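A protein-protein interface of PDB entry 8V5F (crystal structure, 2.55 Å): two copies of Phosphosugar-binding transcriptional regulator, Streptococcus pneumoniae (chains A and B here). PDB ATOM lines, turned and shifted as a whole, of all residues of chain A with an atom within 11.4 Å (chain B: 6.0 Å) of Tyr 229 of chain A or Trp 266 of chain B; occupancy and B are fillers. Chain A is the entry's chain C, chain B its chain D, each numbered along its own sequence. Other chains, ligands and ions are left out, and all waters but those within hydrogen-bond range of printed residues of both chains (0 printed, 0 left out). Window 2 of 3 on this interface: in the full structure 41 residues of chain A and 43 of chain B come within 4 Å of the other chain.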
ATOM      1  N   ARG A  93      23.698   6.599 -33.467  1.00  0.00           N
ATOM      2  CA  ARG A  93      22.334   6.080 -33.491  1.00  0.00           C
ATOM      3  C   ARG A  93      21.710   6.112 -32.100  1.00  0.00           C
ATOM      4  O   ARG A  93      20.558   6.533 -31.926  1.00  0.00           O
ATOM      5  CB  ARG A  93      22.334   4.655 -34.050  1.00  0.00           C
ATOM      6  CG  ARG A  93      21.007   3.921 -33.921  1.00  0.00           C
ATOM      7  CD  ARG A  93      21.135   2.653 -33.074  1.00  0.00           C
ATOM      8  NE  ARG A  93      21.524   1.495 -33.873  1.00  0.00           N
ATOM      9  CZ  ARG A  93      21.847   0.309 -33.375  1.00  0.00           C
ATOM     10  NH1 ARG A  93      21.821   0.076 -32.071  1.00  0.00           N
ATOM     11  NH2 ARG A  93      22.198  -0.669 -34.206  1.00  0.00           N
ATOM     12  N   SER A  97      18.623   8.525 -30.871  1.00  0.00           N
ATOM     13  CA  SER A  97      17.378   8.008 -30.319  1.00  0.00           C
ATOM     14  C   SER A  97      17.006   8.748 -29.046  1.00  0.00           C
ATOM     15  O   SER A  97      15.830   9.050 -28.819  1.00  0.00           O
ATOM     16  CB  SER A  97      17.504   6.514 -30.055  1.00  0.00           C
ATOM     17  OG  SER A  97      17.336   5.768 -31.242  1.00  0.00           O
ATOM     18  N   MET A 101      13.792  11.199 -28.604  1.00  0.00           N
ATOM     19  CA  MET A 101      12.846  11.000 -27.510  1.00  0.00           C
ATOM     20  C   MET A 101      12.571  12.318 -26.799  1.00  0.00           C
ATOM     21  O   MET A 101      11.416  12.645 -26.507  1.00  0.00           O
ATOM     22  CB  MET A 101      13.380   9.964 -26.515  1.00  0.00           C
ATOM     23  CG  MET A 101      12.315   9.408 -25.563  1.00  0.00           C
ATOM     24  SD  MET A 101      12.518   7.644 -25.221  1.00  0.00           S
ATOM     25  CE  MET A 101      11.652   6.912 -26.616  1.00  0.00           C
ATOM     26  N   SER A 134       9.597  -3.770 -18.276  1.00  0.00           N
ATOM     27  CA  SER A 134      10.336  -2.523 -18.107  1.00  0.00           C
ATOM     28  C   SER A 134       9.464  -1.437 -17.486  1.00  0.00           C
ATOM     29  O   SER A 134       9.947  -0.630 -16.682  1.00  0.00           O
ATOM     30  CB  SER A 134      10.903  -2.073 -19.449  1.00  0.00           C
ATOM     31  OG  SER A 134      11.504  -3.167 -20.130  1.00  0.00           O
ATOM     32  N   LEU A 180       3.368   1.007 -22.228  1.00  0.00           N
ATOM     33  CA  LEU A 180       3.920   1.662 -23.408  1.00  0.00           C
ATOM     34  C   LEU A 180       3.106   1.332 -24.650  1.00  0.00           C
ATOM     35  O   LEU A 180       2.874   2.200 -25.499  1.00  0.00           O
ATOM     36  CB  LEU A 180       5.376   1.248 -23.612  1.00  0.00           C
ATOM     37  CG  LEU A 180       6.469   2.266 -23.292  1.00  0.00           C
ATOM     38  CD1 LEU A 180       7.812   1.534 -23.209  1.00  0.00           C
ATOM     39  CD2 LEU A 180       6.509   3.365 -24.323  1.00  0.00           C
ATOM     40  N   SER A 181       2.666   0.080 -24.780  1.00  0.00           N
ATOM     41  CA  SER A 181       1.914  -0.322 -25.963  1.00  0.00           C
ATOM     42  C   SER A 181       0.486   0.210 -25.949  1.00  0.00           C
ATOM     43  O   SER A 181      -0.106   0.415 -27.015  1.00  0.00           O
ATOM     44  CB  SER A 181       1.888  -1.848 -26.077  1.00  0.00           C
ATOM     45  OG  SER A 181       3.101  -2.434 -25.623  1.00  0.00           O
ATOM     46  N   GLY A 182      -0.085   0.431 -24.768  1.00  0.00           N
ATOM     47  CA  GLY A 182      -1.486   0.773 -24.664  1.00  0.00           C
ATOM     48  C   GLY A 182      -2.431  -0.392 -24.829  1.00  0.00           C
ATOM     49  O   GLY A 182      -3.647  -0.178 -24.883  1.00  0.00           O
ATOM     50  N   SER A 183      -1.910  -1.620 -24.912  1.00  0.00           N
ATOM     51  CA  SER A 183      -2.753  -2.796 -25.072  1.00  0.00           C
ATOM     52  C   SER A 183      -2.320  -3.951 -24.174  1.00  0.00           C
ATOM     53  O   SER A 183      -2.849  -5.060 -24.326  1.00  0.00           O
ATOM     54  CB  SER A 183      -2.759  -3.253 -26.539  1.00  0.00           C
ATOM     55  OG  SER A 183      -3.868  -2.709 -27.237  1.00  0.00           O
ATOM     56  N   THR A 184      -1.375  -3.736 -23.257  1.00  0.00           N
ATOM     57  CA  THR A 184      -1.027  -4.743 -22.263  1.00  0.00           C
ATOM     58  C   THR A 184      -2.273  -4.998 -21.421  1.00  0.00           C
ATOM     59  O   THR A 184      -2.676  -4.136 -20.625  1.00  0.00           O
ATOM     60  CB  THR A 184       0.146  -4.283 -21.395  1.00  0.00           C
ATOM     61  OG1 THR A 184       0.044  -2.875 -21.154  1.00  0.00           O
ATOM     62  CG2 THR A 184       1.481  -4.584 -22.091  1.00  0.00           C
ATOM     63  N   SER A 206       2.283   5.182 -25.343  1.00  0.00           N
ATOM     64  CA  SER A 206       2.758   5.752 -26.596  1.00  0.00           C
ATOM     65  C   SER A 206       1.701   5.711 -27.691  1.00  0.00           C
ATOM     66  O   SER A 206       1.868   6.388 -28.713  1.00  0.00           O
ATOM     67  CB  SER A 206       4.011   5.013 -27.081  1.00  0.00           C
ATOM     68  OG  SER A 206       3.678   3.812 -27.761  1.00  0.00           O
ATOM     69  N   VAL A 207       0.640   4.939 -27.502  1.00  0.00           N
ATOM     70  CA  VAL A 207      -0.482   4.839 -28.436  1.00  0.00           C
ATOM     71  C   VAL A 207      -1.663   5.586 -27.837  1.00  0.00           C
ATOM     72  O   VAL A 207      -1.970   5.389 -26.654  1.00  0.00           O
ATOM     73  CB  VAL A 207      -0.861   3.370 -28.714  1.00  0.00           C
ATOM     74  CG1 VAL A 207      -1.750   3.266 -29.952  1.00  0.00           C
ATOM     75  CG2 VAL A 207       0.391   2.514 -28.860  1.00  0.00           C
ATOM     76  N   THR A 223       7.104   7.974 -28.631  1.00  0.00           N
ATOM     77  CA  THR A 223       7.342   6.729 -29.341  1.00  0.00           C
ATOM     78  C   THR A 223       8.822   6.609 -29.688  1.00  0.00           C
ATOM     79  O   THR A 223       9.499   7.601 -29.974  1.00  0.00           O
ATOM     80  CB  THR A 223       6.494   6.653 -30.613  1.00  0.00           C
ATOM     81  OG1 THR A 223       5.104   6.577 -30.260  1.00  0.00           O
ATOM     82  CG2 THR A 223       6.889   5.431 -31.447  1.00  0.00           C
ATOM     83  N   HIS A 224       9.320   5.376 -29.654  1.00  0.00           N
ATOM     84  CA  HIS A 224      10.736   5.133 -29.894  1.00  0.00           C
ATOM     85  C   HIS A 224      11.120   5.488 -31.327  1.00  0.00           C
ATOM     86  O   HIS A 224      10.369   5.231 -32.274  1.00  0.00           O
ATOM     87  CB  HIS A 224      11.070   3.665 -29.628  1.00  0.00           C
ATOM     88  CG  HIS A 224      11.169   3.322 -28.177  1.00  0.00           C
ATOM     89  ND1 HIS A 224      12.339   3.446 -27.459  1.00  0.00           N
ATOM     90  CD2 HIS A 224      10.243   2.854 -27.309  1.00  0.00           C
ATOM     91  CE1 HIS A 224      12.125   3.077 -26.207  1.00  0.00           C
ATOM     92  NE2 HIS A 224      10.860   2.718 -26.090  1.00  0.00           N
ATOM     93  N   SER A 225      12.313   6.065 -31.488  1.00  0.00           N
ATOM     94  CA  SER A 225      12.769   6.428 -32.827  1.00  0.00           C
ATOM     95  C   SER A 225      13.007   5.187 -33.682  1.00  0.00           C
ATOM     96  O   SER A 225      12.556   5.116 -34.831  1.00  0.00           O
ATOM     97  CB  SER A 225      14.039   7.280 -32.744  1.00  0.00           C
ATOM     98  OG  SER A 225      14.065   8.053 -31.558  1.00  0.00           O
ATOM     99  N   GLN A 226      13.706   4.193 -33.136  1.00  0.00           N
ATOM    100  CA  GLN A 226      14.054   3.022 -33.927  1.00  0.00           C
ATOM    101  C   GLN A 226      12.800   2.211 -34.245  1.00  0.00           C
ATOM    102  O   GLN A 226      11.947   2.017 -33.371  1.00  0.00           O
ATOM    103  CB  GLN A 226      15.059   2.145 -33.184  1.00  0.00           C
ATOM    104  CG  GLN A 226      16.475   2.697 -33.133  1.00  0.00           C
ATOM    105  CD  GLN A 226      17.170   2.656 -34.484  1.00  0.00           C
ATOM    106  OE1 GLN A 226      16.960   1.739 -35.281  1.00  0.00           O
ATOM    107  NE2 GLN A 226      18.013   3.649 -34.744  1.00  0.00           N
ATOM    108  N   PRO A 227      12.665   1.701 -35.473  1.00  0.00           N
ATOM    109  CA  PRO A 227      11.485   0.889 -35.794  1.00  0.00           C
ATOM    110  C   PRO A 227      11.568  -0.516 -35.219  1.00  0.00           C
ATOM    111  O   PRO A 227      10.577  -1.034 -34.690  1.00  0.00           O
ATOM    112  CB  PRO A 227      11.463   0.864 -37.329  1.00  0.00           C
ATOM    113  CG  PRO A 227      12.805   1.386 -37.788  1.00  0.00           C
ATOM    114  CD  PRO A 227      13.630   1.760 -36.587  1.00  0.00           C
ATOM    115  N   SER A 228      12.744  -1.139 -35.305  1.00  0.00           N
ATOM    116  CA  SER A 228      12.905  -2.534 -34.908  1.00  0.00           C
ATOM    117  C   SER A 228      13.004  -2.671 -33.392  1.00  0.00           C
ATOM    118  O   SER A 228      13.816  -1.995 -32.752  1.00  0.00           O
ATOM    119  CB  SER A 228      14.155  -3.120 -35.563  1.00  0.00           C
ATOM    120  OG  SER A 228      15.222  -2.182 -35.570  1.00  0.00           O
ATOM    121  N   TYR A 229      12.205  -3.585 -32.824  1.00  0.00           N
ATOM    122  CA  TYR A 229      12.168  -3.747 -31.372  1.00  0.00           C
ATOM    123  C   TYR A 229      13.560  -3.990 -30.807  1.00  0.00           C
ATOM    124  O   TYR A 229      13.930  -3.432 -29.764  1.00  0.00           O
ATOM    125  CB  TYR A 229      11.252  -4.913 -30.989  1.00  0.00           C
ATOM    126  CG  TYR A 229       9.796  -4.759 -31.374  1.00  0.00           C
ATOM    127  CD1 TYR A 229       9.107  -3.580 -31.127  1.00  0.00           C
ATOM    128  CD2 TYR A 229       9.108  -5.804 -31.984  1.00  0.00           C
ATOM    129  CE1 TYR A 229       7.775  -3.444 -31.475  1.00  0.00           C
ATOM    130  CE2 TYR A 229       7.780  -5.675 -32.343  1.00  0.00           C
ATOM    131  CZ  TYR A 229       7.118  -4.490 -32.086  1.00  0.00           C
ATOM    132  OH  TYR A 229       5.792  -4.347 -32.431  1.00  0.00           O
ATOM    133  N   ILE A 230      14.348  -4.827 -31.484  1.00  0.00           N
ATOM    134  CA  ILE A 230      15.625  -5.248 -30.927  1.00  0.00           C
ATOM    135  C   ILE A 230      16.589  -4.076 -30.825  1.00  0.00           C
ATOM    136  O   ILE A 230      17.408  -4.022 -29.899  1.00  0.00           O
ATOM    137  CB  ILE A 230      16.207  -6.406 -31.761  1.00  0.00           C
ATOM    138  CG1 ILE A 230      17.589  -6.815 -31.242  1.00  0.00           C
ATOM    139  CG2 ILE A 230      16.299  -6.026 -33.228  1.00  0.00           C
ATOM    140  CD1 ILE A 230      17.834  -8.311 -31.280  1.00  0.00           C
ATOM    141  N   GLN A 231      16.520  -3.125 -31.758  1.00  0.00           N
ATOM    142  CA  GLN A 231      17.472  -2.019 -31.817  1.00  0.00           C
ATOM    143  C   GLN A 231      17.049  -0.816 -30.987  1.00  0.00           C
ATOM    144  O   GLN A 231      17.810   0.155 -30.898  1.00  0.00           O
ATOM    145  CB  GLN A 231      17.683  -1.582 -33.272  1.00  0.00           C
ATOM    146  CG  GLN A 231      18.251  -2.683 -34.154  1.00  0.00           C
ATOM    147  CD  GLN A 231      19.033  -2.157 -35.340  1.00  0.00           C
ATOM    148  OE1 GLN A 231      20.103  -1.569 -35.184  1.00  0.00           O
ATOM    149  NE2 GLN A 231      18.501  -2.372 -36.540  1.00  0.00           N
ATOM    150  N   ARG A 232      15.872  -0.858 -30.371  1.00  0.00           N
ATOM    151  CA  ARG A 232      15.378   0.284 -29.617  1.00  0.00           C
ATOM    152  C   ARG A 232      16.222   0.518 -28.374  1.00  0.00           C
ATOM    153  O   ARG A 232      16.819  -0.407 -27.814  1.00  0.00           O
ATOM    154  CB  ARG A 232      13.929   0.064 -29.188  1.00  0.00           C
ATOM    155  CG  ARG A 232      12.964  -0.184 -30.320  1.00  0.00           C
ATOM    156  CD  ARG A 232      11.583   0.272 -29.915  1.00  0.00           C
ATOM    157  NE  ARG A 232      10.548  -0.106 -30.867  1.00  0.00           N
ATOM    158  CZ  ARG A 232       9.254  -0.133 -30.575  1.00  0.00           C
ATOM    159  NH1 ARG A 232       8.814   0.158 -29.362  1.00  0.00           N
ATOM    160  NH2 ARG A 232       8.381  -0.463 -31.523  1.00  0.00           N
ATOM    161  N   ILE A 233      16.265   1.776 -27.944  1.00  0.00           N
ATOM    162  CA  ILE A 233      16.847   2.135 -26.655  1.00  0.00           C
ATOM    163  C   ILE A 233      15.885   1.699 -25.557  1.00  0.00           C
ATOM    164  O   ILE A 233      14.812   1.148 -25.833  1.00  0.00           O
ATOM    165  CB  ILE A 233      17.145   3.643 -26.567  1.00  0.00           C
ATOM    166  CG1 ILE A 233      15.870   4.472 -26.784  1.00  0.00           C
ATOM    167  CG2 ILE A 233      18.210   4.020 -27.576  1.00  0.00           C
ATOM    168  CD1 ILE A 233      15.798   5.720 -25.928  1.00  0.00           C
ATOM    169  N   SER A 234      16.250   1.972 -24.310  1.00  0.00           N
ATOM    170  CA  SER A 234      15.495   1.463 -23.176  1.00  0.00           C
ATOM    171  C   SER A 234      14.017   1.799 -23.288  1.00  0.00           C
ATOM    172  O   SER A 234      13.643   2.949 -23.532  1.00  0.00           O
ATOM    173  CB  SER A 234      16.065   2.049 -21.888  1.00  0.00           C
ATOM    174  OG  SER A 234      15.128   1.949 -20.831  1.00  0.00           O
ATOM    175  N   ALA A 235      13.177   0.780 -23.085  1.00  0.00           N
ATOM    176  CA  ALA A 235      11.733   0.993 -23.063  1.00  0.00           C
ATOM    177  C   ALA A 235      11.294   1.824 -21.865  1.00  0.00           C
ATOM    178  O   ALA A 235      10.199   2.395 -21.889  1.00  0.00           O
ATOM    179  CB  ALA A 235      10.993  -0.348 -23.054  1.00  0.00           C
ATOM    180  N   GLN A 236      12.122   1.911 -20.821  1.00  0.00           N
ATOM    181  CA  GLN A 236      11.781   2.751 -19.678  1.00  0.00           C
ATOM    182  C   GLN A 236      11.620   4.212 -20.098  1.00  0.00           C
ATOM    183  O   GLN A 236      10.688   4.891 -19.653  1.00  0.00           O
ATOM    184  CB  GLN A 236      12.862   2.641 -18.594  1.00  0.00           C
ATOM    185  CG  GLN A 236      12.665   1.548 -17.547  1.00  0.00           C
ATOM    186  CD  GLN A 236      13.601   1.689 -16.337  1.00  0.00           C
ATOM    187  OE1 GLN A 236      13.292   2.386 -15.371  1.00  0.00           O
ATOM    188  NE2 GLN A 236      14.761   1.046 -16.407  1.00  0.00           N
ATOM    189  N   ARG B 145      17.281  -6.934 -20.847  1.00  0.00           N
ATOM    190  CA  ARG B 145      17.645  -6.717 -22.248  1.00  0.00           C
ATOM    191  C   ARG B 145      18.628  -7.771 -22.731  1.00  0.00           C
ATOM    192  O   ARG B 145      18.542  -8.231 -23.874  1.00  0.00           O
ATOM    193  CB  ARG B 145      18.268  -5.332 -22.470  1.00  0.00           C
ATOM    194  CG  ARG B 145      17.369  -4.179 -22.132  1.00  0.00           C
ATOM    195  CD  ARG B 145      16.280  -3.959 -23.161  1.00  0.00           C
ATOM    196  NE  ARG B 145      16.762  -3.802 -24.526  1.00  0.00           N
ATOM    197  CZ  ARG B 145      17.268  -2.675 -25.017  1.00  0.00           C
ATOM    198  NH1 ARG B 145      17.674  -1.694 -24.226  1.00  0.00           N
ATOM    199  NH2 ARG B 145      17.378  -2.531 -26.335  1.00  0.00           N
ATOM    200  N   ARG B 148      17.591 -11.567 -23.363  1.00  0.00           N
ATOM    201  CA  ARG B 148      16.864 -11.762 -24.607  1.00  0.00           C
ATOM    202  C   ARG B 148      17.784 -11.763 -25.813  1.00  0.00           C
ATOM    203  O   ARG B 148      17.315 -11.960 -26.938  1.00  0.00           O
ATOM    204  CB  ARG B 148      15.799 -10.680 -24.750  1.00  0.00           C
ATOM    205  CG  ARG B 148      15.006 -10.480 -23.474  1.00  0.00           C
ATOM    206  CD  ARG B 148      14.010  -9.369 -23.613  1.00  0.00           C
ATOM    207  NE  ARG B 148      13.150  -9.585 -24.767  1.00  0.00           N
ATOM    208  CZ  ARG B 148      12.170  -8.771 -25.135  1.00  0.00           C
ATOM    209  NH1 ARG B 148      11.892  -7.670 -24.453  1.00  0.00           N
ATOM    210  NH2 ARG B 148      11.452  -9.071 -26.211  1.00  0.00           N
ATOM    211  N   TYR B 247      24.748  -2.136 -25.235  1.00  0.00           N
ATOM    212  CA  TYR B 247      23.840  -3.065 -25.896  1.00  0.00           C
ATOM    213  C   TYR B 247      23.980  -2.977 -27.410  1.00  0.00           C
ATOM    214  O   TYR B 247      24.054  -4.002 -28.099  1.00  0.00           O
ATOM    215  CB  TYR B 247      22.411  -2.761 -25.466  1.00  0.00           C
ATOM    216  CG  TYR B 247      21.340  -3.553 -26.173  1.00  0.00           C
ATOM    217  CD1 TYR B 247      20.861  -3.158 -27.414  1.00  0.00           C
ATOM    218  CD2 TYR B 247      20.788  -4.681 -25.584  1.00  0.00           C
ATOM    219  CE1 TYR B 247      19.868  -3.877 -28.053  1.00  0.00           C
ATOM    220  CE2 TYR B 247      19.798  -5.401 -26.213  1.00  0.00           C
ATOM    221  CZ  TYR B 247      19.335  -4.996 -27.443  1.00  0.00           C
ATOM    222  OH  TYR B 247      18.342  -5.720 -28.065  1.00  0.00           O
ATOM    223  N   PHE B 262      16.248 -13.403 -29.711  1.00  0.00           N
ATOM    224  CA  PHE B 262      15.302 -12.321 -29.484  1.00  0.00           C
ATOM    225  C   PHE B 262      13.944 -12.672 -30.074  1.00  0.00           C
ATOM    226  O   PHE B 262      12.917 -12.591 -29.388  1.00  0.00           O
ATOM    227  CB  PHE B 262      15.840 -11.022 -30.077  1.00  0.00           C
ATOM    228  CG  PHE B 262      15.090  -9.795 -29.637  1.00  0.00           C
ATOM    229  CD1 PHE B 262      15.385  -9.179 -28.429  1.00  0.00           C
ATOM    230  CD2 PHE B 262      14.108  -9.244 -30.440  1.00  0.00           C
ATOM    231  CE1 PHE B 262      14.703  -8.049 -28.033  1.00  0.00           C
ATOM    232  CE2 PHE B 262      13.438  -8.110 -30.054  1.00  0.00           C
ATOM    233  CZ  PHE B 262      13.727  -7.515 -28.847  1.00  0.00           C
ATOM    234  N   ASN B 263      13.927 -13.122 -31.332  1.00  0.00           N
ATOM    235  CA  ASN B 263      12.668 -13.388 -32.016  1.00  0.00           C
ATOM    236  C   ASN B 263      12.020 -14.692 -31.573  1.00  0.00           C
ATOM    237  O   ASN B 263      10.825 -14.886 -31.824  1.00  0.00           O
ATOM    238  CB  ASN B 263      12.889 -13.397 -33.532  1.00  0.00           C
ATOM    239  CG  ASN B 263      13.378 -12.057 -34.057  1.00  0.00           C
ATOM    240  OD1 ASN B 263      13.020 -11.000 -33.532  1.00  0.00           O
ATOM    241  ND2 ASN B 263      14.217 -12.094 -35.085  1.00  0.00           N
ATOM    242  N   SER B 264      12.767 -15.579 -30.908  1.00  0.00           N
ATOM    243  CA  SER B 264      12.163 -16.803 -30.394  1.00  0.00           C
ATOM    244  C   SER B 264      11.091 -16.487 -29.360  1.00  0.00           C
ATOM    245  O   SER B 264      10.123 -17.248 -29.219  1.00  0.00           O
ATOM    246  CB  SER B 264      13.240 -17.711 -29.796  1.00  0.00           C
ATOM    247  OG  SER B 264      14.133 -16.966 -28.990  1.00  0.00           O
ATOM    248  N   TYR B 265      11.235 -15.364 -28.643  1.00  0.00           N
ATOM    249  CA  TYR B 265      10.230 -14.967 -27.661  1.00  0.00           C
ATOM    250  C   TYR B 265       8.883 -14.773 -28.329  1.00  0.00           C
ATOM    251  O   TYR B 265       7.853 -15.234 -27.826  1.00  0.00           O
ATOM    252  CB  TYR B 265      10.664 -13.686 -26.946  1.00  0.00           C
ATOM    253  CG  TYR B 265       9.519 -12.887 -26.345  1.00  0.00           C
ATOM    254  CD1 TYR B 265       9.279 -12.920 -24.991  1.00  0.00           C
ATOM    255  CD2 TYR B 265       8.678 -12.096 -27.141  1.00  0.00           C
ATOM    256  CE1 TYR B 265       8.257 -12.199 -24.438  1.00  0.00           C
ATOM    257  CE2 TYR B 265       7.626 -11.382 -26.591  1.00  0.00           C
ATOM    258  CZ  TYR B 265       7.433 -11.427 -25.238  1.00  0.00           C
ATOM    259  OH  TYR B 265       6.404 -10.706 -24.682  1.00  0.00           O
ATOM    260  N   TRP B 266       8.884 -14.117 -29.494  1.00  0.00           N
ATOM    261  CA  TRP B 266       7.645 -13.919 -30.233  1.00  0.00           C
ATOM    262  C   TRP B 266       7.126 -15.239 -30.785  1.00  0.00           C
ATOM    263  O   TRP B 266       5.920 -15.507 -30.730  1.00  0.00           O
ATOM    264  CB  TRP B 266       7.857 -12.911 -31.360  1.00  0.00           C
ATOM    265  CG  TRP B 266       7.864 -11.492 -30.886  1.00  0.00           C
ATOM    266  CD1 TRP B 266       6.850 -10.583 -30.991  1.00  0.00           C
ATOM    267  CD2 TRP B 266       8.936 -10.821 -30.218  1.00  0.00           C
ATOM    268  NE1 TRP B 266       7.231  -9.385 -30.436  1.00  0.00           N
ATOM    269  CE2 TRP B 266       8.505  -9.507 -29.951  1.00  0.00           C
ATOM    270  CE3 TRP B 266      10.221 -11.204 -29.823  1.00  0.00           C
ATOM    271  CZ2 TRP B 266       9.311  -8.574 -29.307  1.00  0.00           C
ATOM    272  CZ3 TRP B 266      11.018 -10.277 -29.181  1.00  0.00           C
ATOM    273  CH2 TRP B 266      10.563  -8.975 -28.939  1.00  0.00           C
ATOM    274  N   GLU B 267       8.029 -16.079 -31.295  1.00  0.00           N
ATOM    275  CA  GLU B 267       7.668 -17.373 -31.860  1.00  0.00           C
ATOM    276  C   GLU B 267       6.865 -18.203 -30.857  1.00  0.00           C
ATOM    277  O   GLU B 267       6.953 -18.023 -29.637  1.00  0.00           O
ATOM    278  CB  GLU B 267       8.929 -18.126 -32.290  1.00  0.00           C
ATOM    279  CG  GLU B 267       8.695 -19.199 -33.341  1.00  0.00           C
ATOM    280  CD  GLU B 267       9.558 -20.418 -33.109  1.00  0.00           C
ATOM    281  OE1 GLU B 267      10.787 -20.314 -33.309  1.00  0.00           O
ATOM    282  OE2 GLU B 267       9.010 -21.477 -32.732  1.00  0.00           O
ATOM    283  N   ASN B 268       6.049 -19.101 -31.400  1.00  0.00           N
ATOM    284  CA  ASN B 268       5.197 -19.973 -30.602  1.00  0.00           C
ATOM    285  C   ASN B 268       5.759 -21.394 -30.559  1.00  0.00           C
ATOM    286  O   ASN B 268       6.514 -21.808 -31.439  1.00  0.00           O
ATOM    287  CB  ASN B 268       3.773 -19.976 -31.168  1.00  0.00           C
ATOM    288  CG  ASN B 268       3.012 -18.698 -30.850  1.00  0.00           C
ATOM    289  OD1 ASN B 268       3.523 -17.592 -31.038  1.00  0.00           O
ATOM    290  ND2 ASN B 268       1.781 -18.845 -30.374  1.00  0.00           N
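Ser 183 of chain A touches none of the printed residues of chain B. Pro 227 of chain A touches none of the printed residues of chain B. Printed residues of chain B within 4 Å of Tyr 229 of chain A: Phe 262 (3.98 Å) and Trp 266 (3.9 Å). Printed residues of chain A within 4 Å of Arg 145 of chain B: Ile 230 (3.9 Å), Arg 232 (2.6 Å) and Ser 234 (3.9 Å). Printed residues of chain A within 4 Å of Tyr 247 of chain B: Ile 230 (2.7 Å). Of the printed residues of chain A, Phe 262 of chain B touches Tyr 229 (3.98 Å) and Ile 230 (3.5 Å). No residue of chain A comes within 4 Å of Asn 263 of chain B. No residue of chain A comes within 4 Å of Tyr 265 of chain B. Trp 266 of chain B touches just one residue of chain A: Tyr 229. No residue of chain A comes within 4 Å of Glu 267 of chain B. No residue of chain A comes within 4 Å of Asn 268 of chain B. The nearest printed residue of chain B that does not touch Tyr 229 of chain A is Arg 145 of chain B (4.9 Å). The nearest residue of chain A that does not touch Trp 266 of chain B is Ile 230 of chain A (6.2 Å).
O of Ile 230 of chain A lies within hydrogen-bond range of OH of Tyr 247 of chain B, at 2.7 Å. The guanidinium group (NH2) of Arg 145 of chain B sits at hydrogen-bond distance from the backbone carbonyl oxygen (O) of Arg 232 of chain A, at 2.6 Å.
Printed residues of chain B that touch a printed residue of chain A: Arg 145, Tyr 247, Phe 262 and Trp 266. Hydrophobic or aromatic side chains of chain B that line the printed part of chain A: Tyr 247, Phe 262 and Trp 266. Along chain B the printed residues that touch a printed residue of chain A span positions 145 to 266. Of the 25 printed residues of chain A, 4 touch a printed residue of chain B. Printed residues of chain A that touch a printed residue of chain B: Tyr 229, Ile 230, Arg 232 and Ser 234. Hydrophobic or aromatic side chains of chain A within 4 Å of the printed part of chain B: Tyr 229 and Ile 230. Among the printed residues, 7 pairs touch across the chains. Among the printed residues, no Asp or Glu carboxylate lies within 4 Å of a Lys or Arg side-chain nitrogen of the other chain.
The side-chain hydroxyl (OG) of Ser 234 of chain A is in hydrogen-bond range of the backbone NH (N) of Gln 236 of chain A (3.0 Å). The backbone carbonyl oxygen (O) of Arg 148 of chain B lies close to the backbone NH (N) of Phe 262 of chain B (3.3 Å). O of Trp 266 of chain B lies close to OD1 of Asn 268 of chain B.
No position is printed for both chains. Of the 7 pairs that touch across the chains among the printed residues, none has its exchanged pair printed and touching as well.
Among the printed residues, merely in contact across the chains: Ile 230 of chain A with Phe 262 of chain B (3.5 Å), Tyr 229 of chain A with Trp 266 of chain B (3.9 Å), Ile 230 of chain A with Arg 145 of chain B (3.9 Å), Ser 234 of chain A with Arg 145 of chain B (3.9 Å) and Tyr 229 of chain A with Phe 262 of chain B (3.98 Å).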
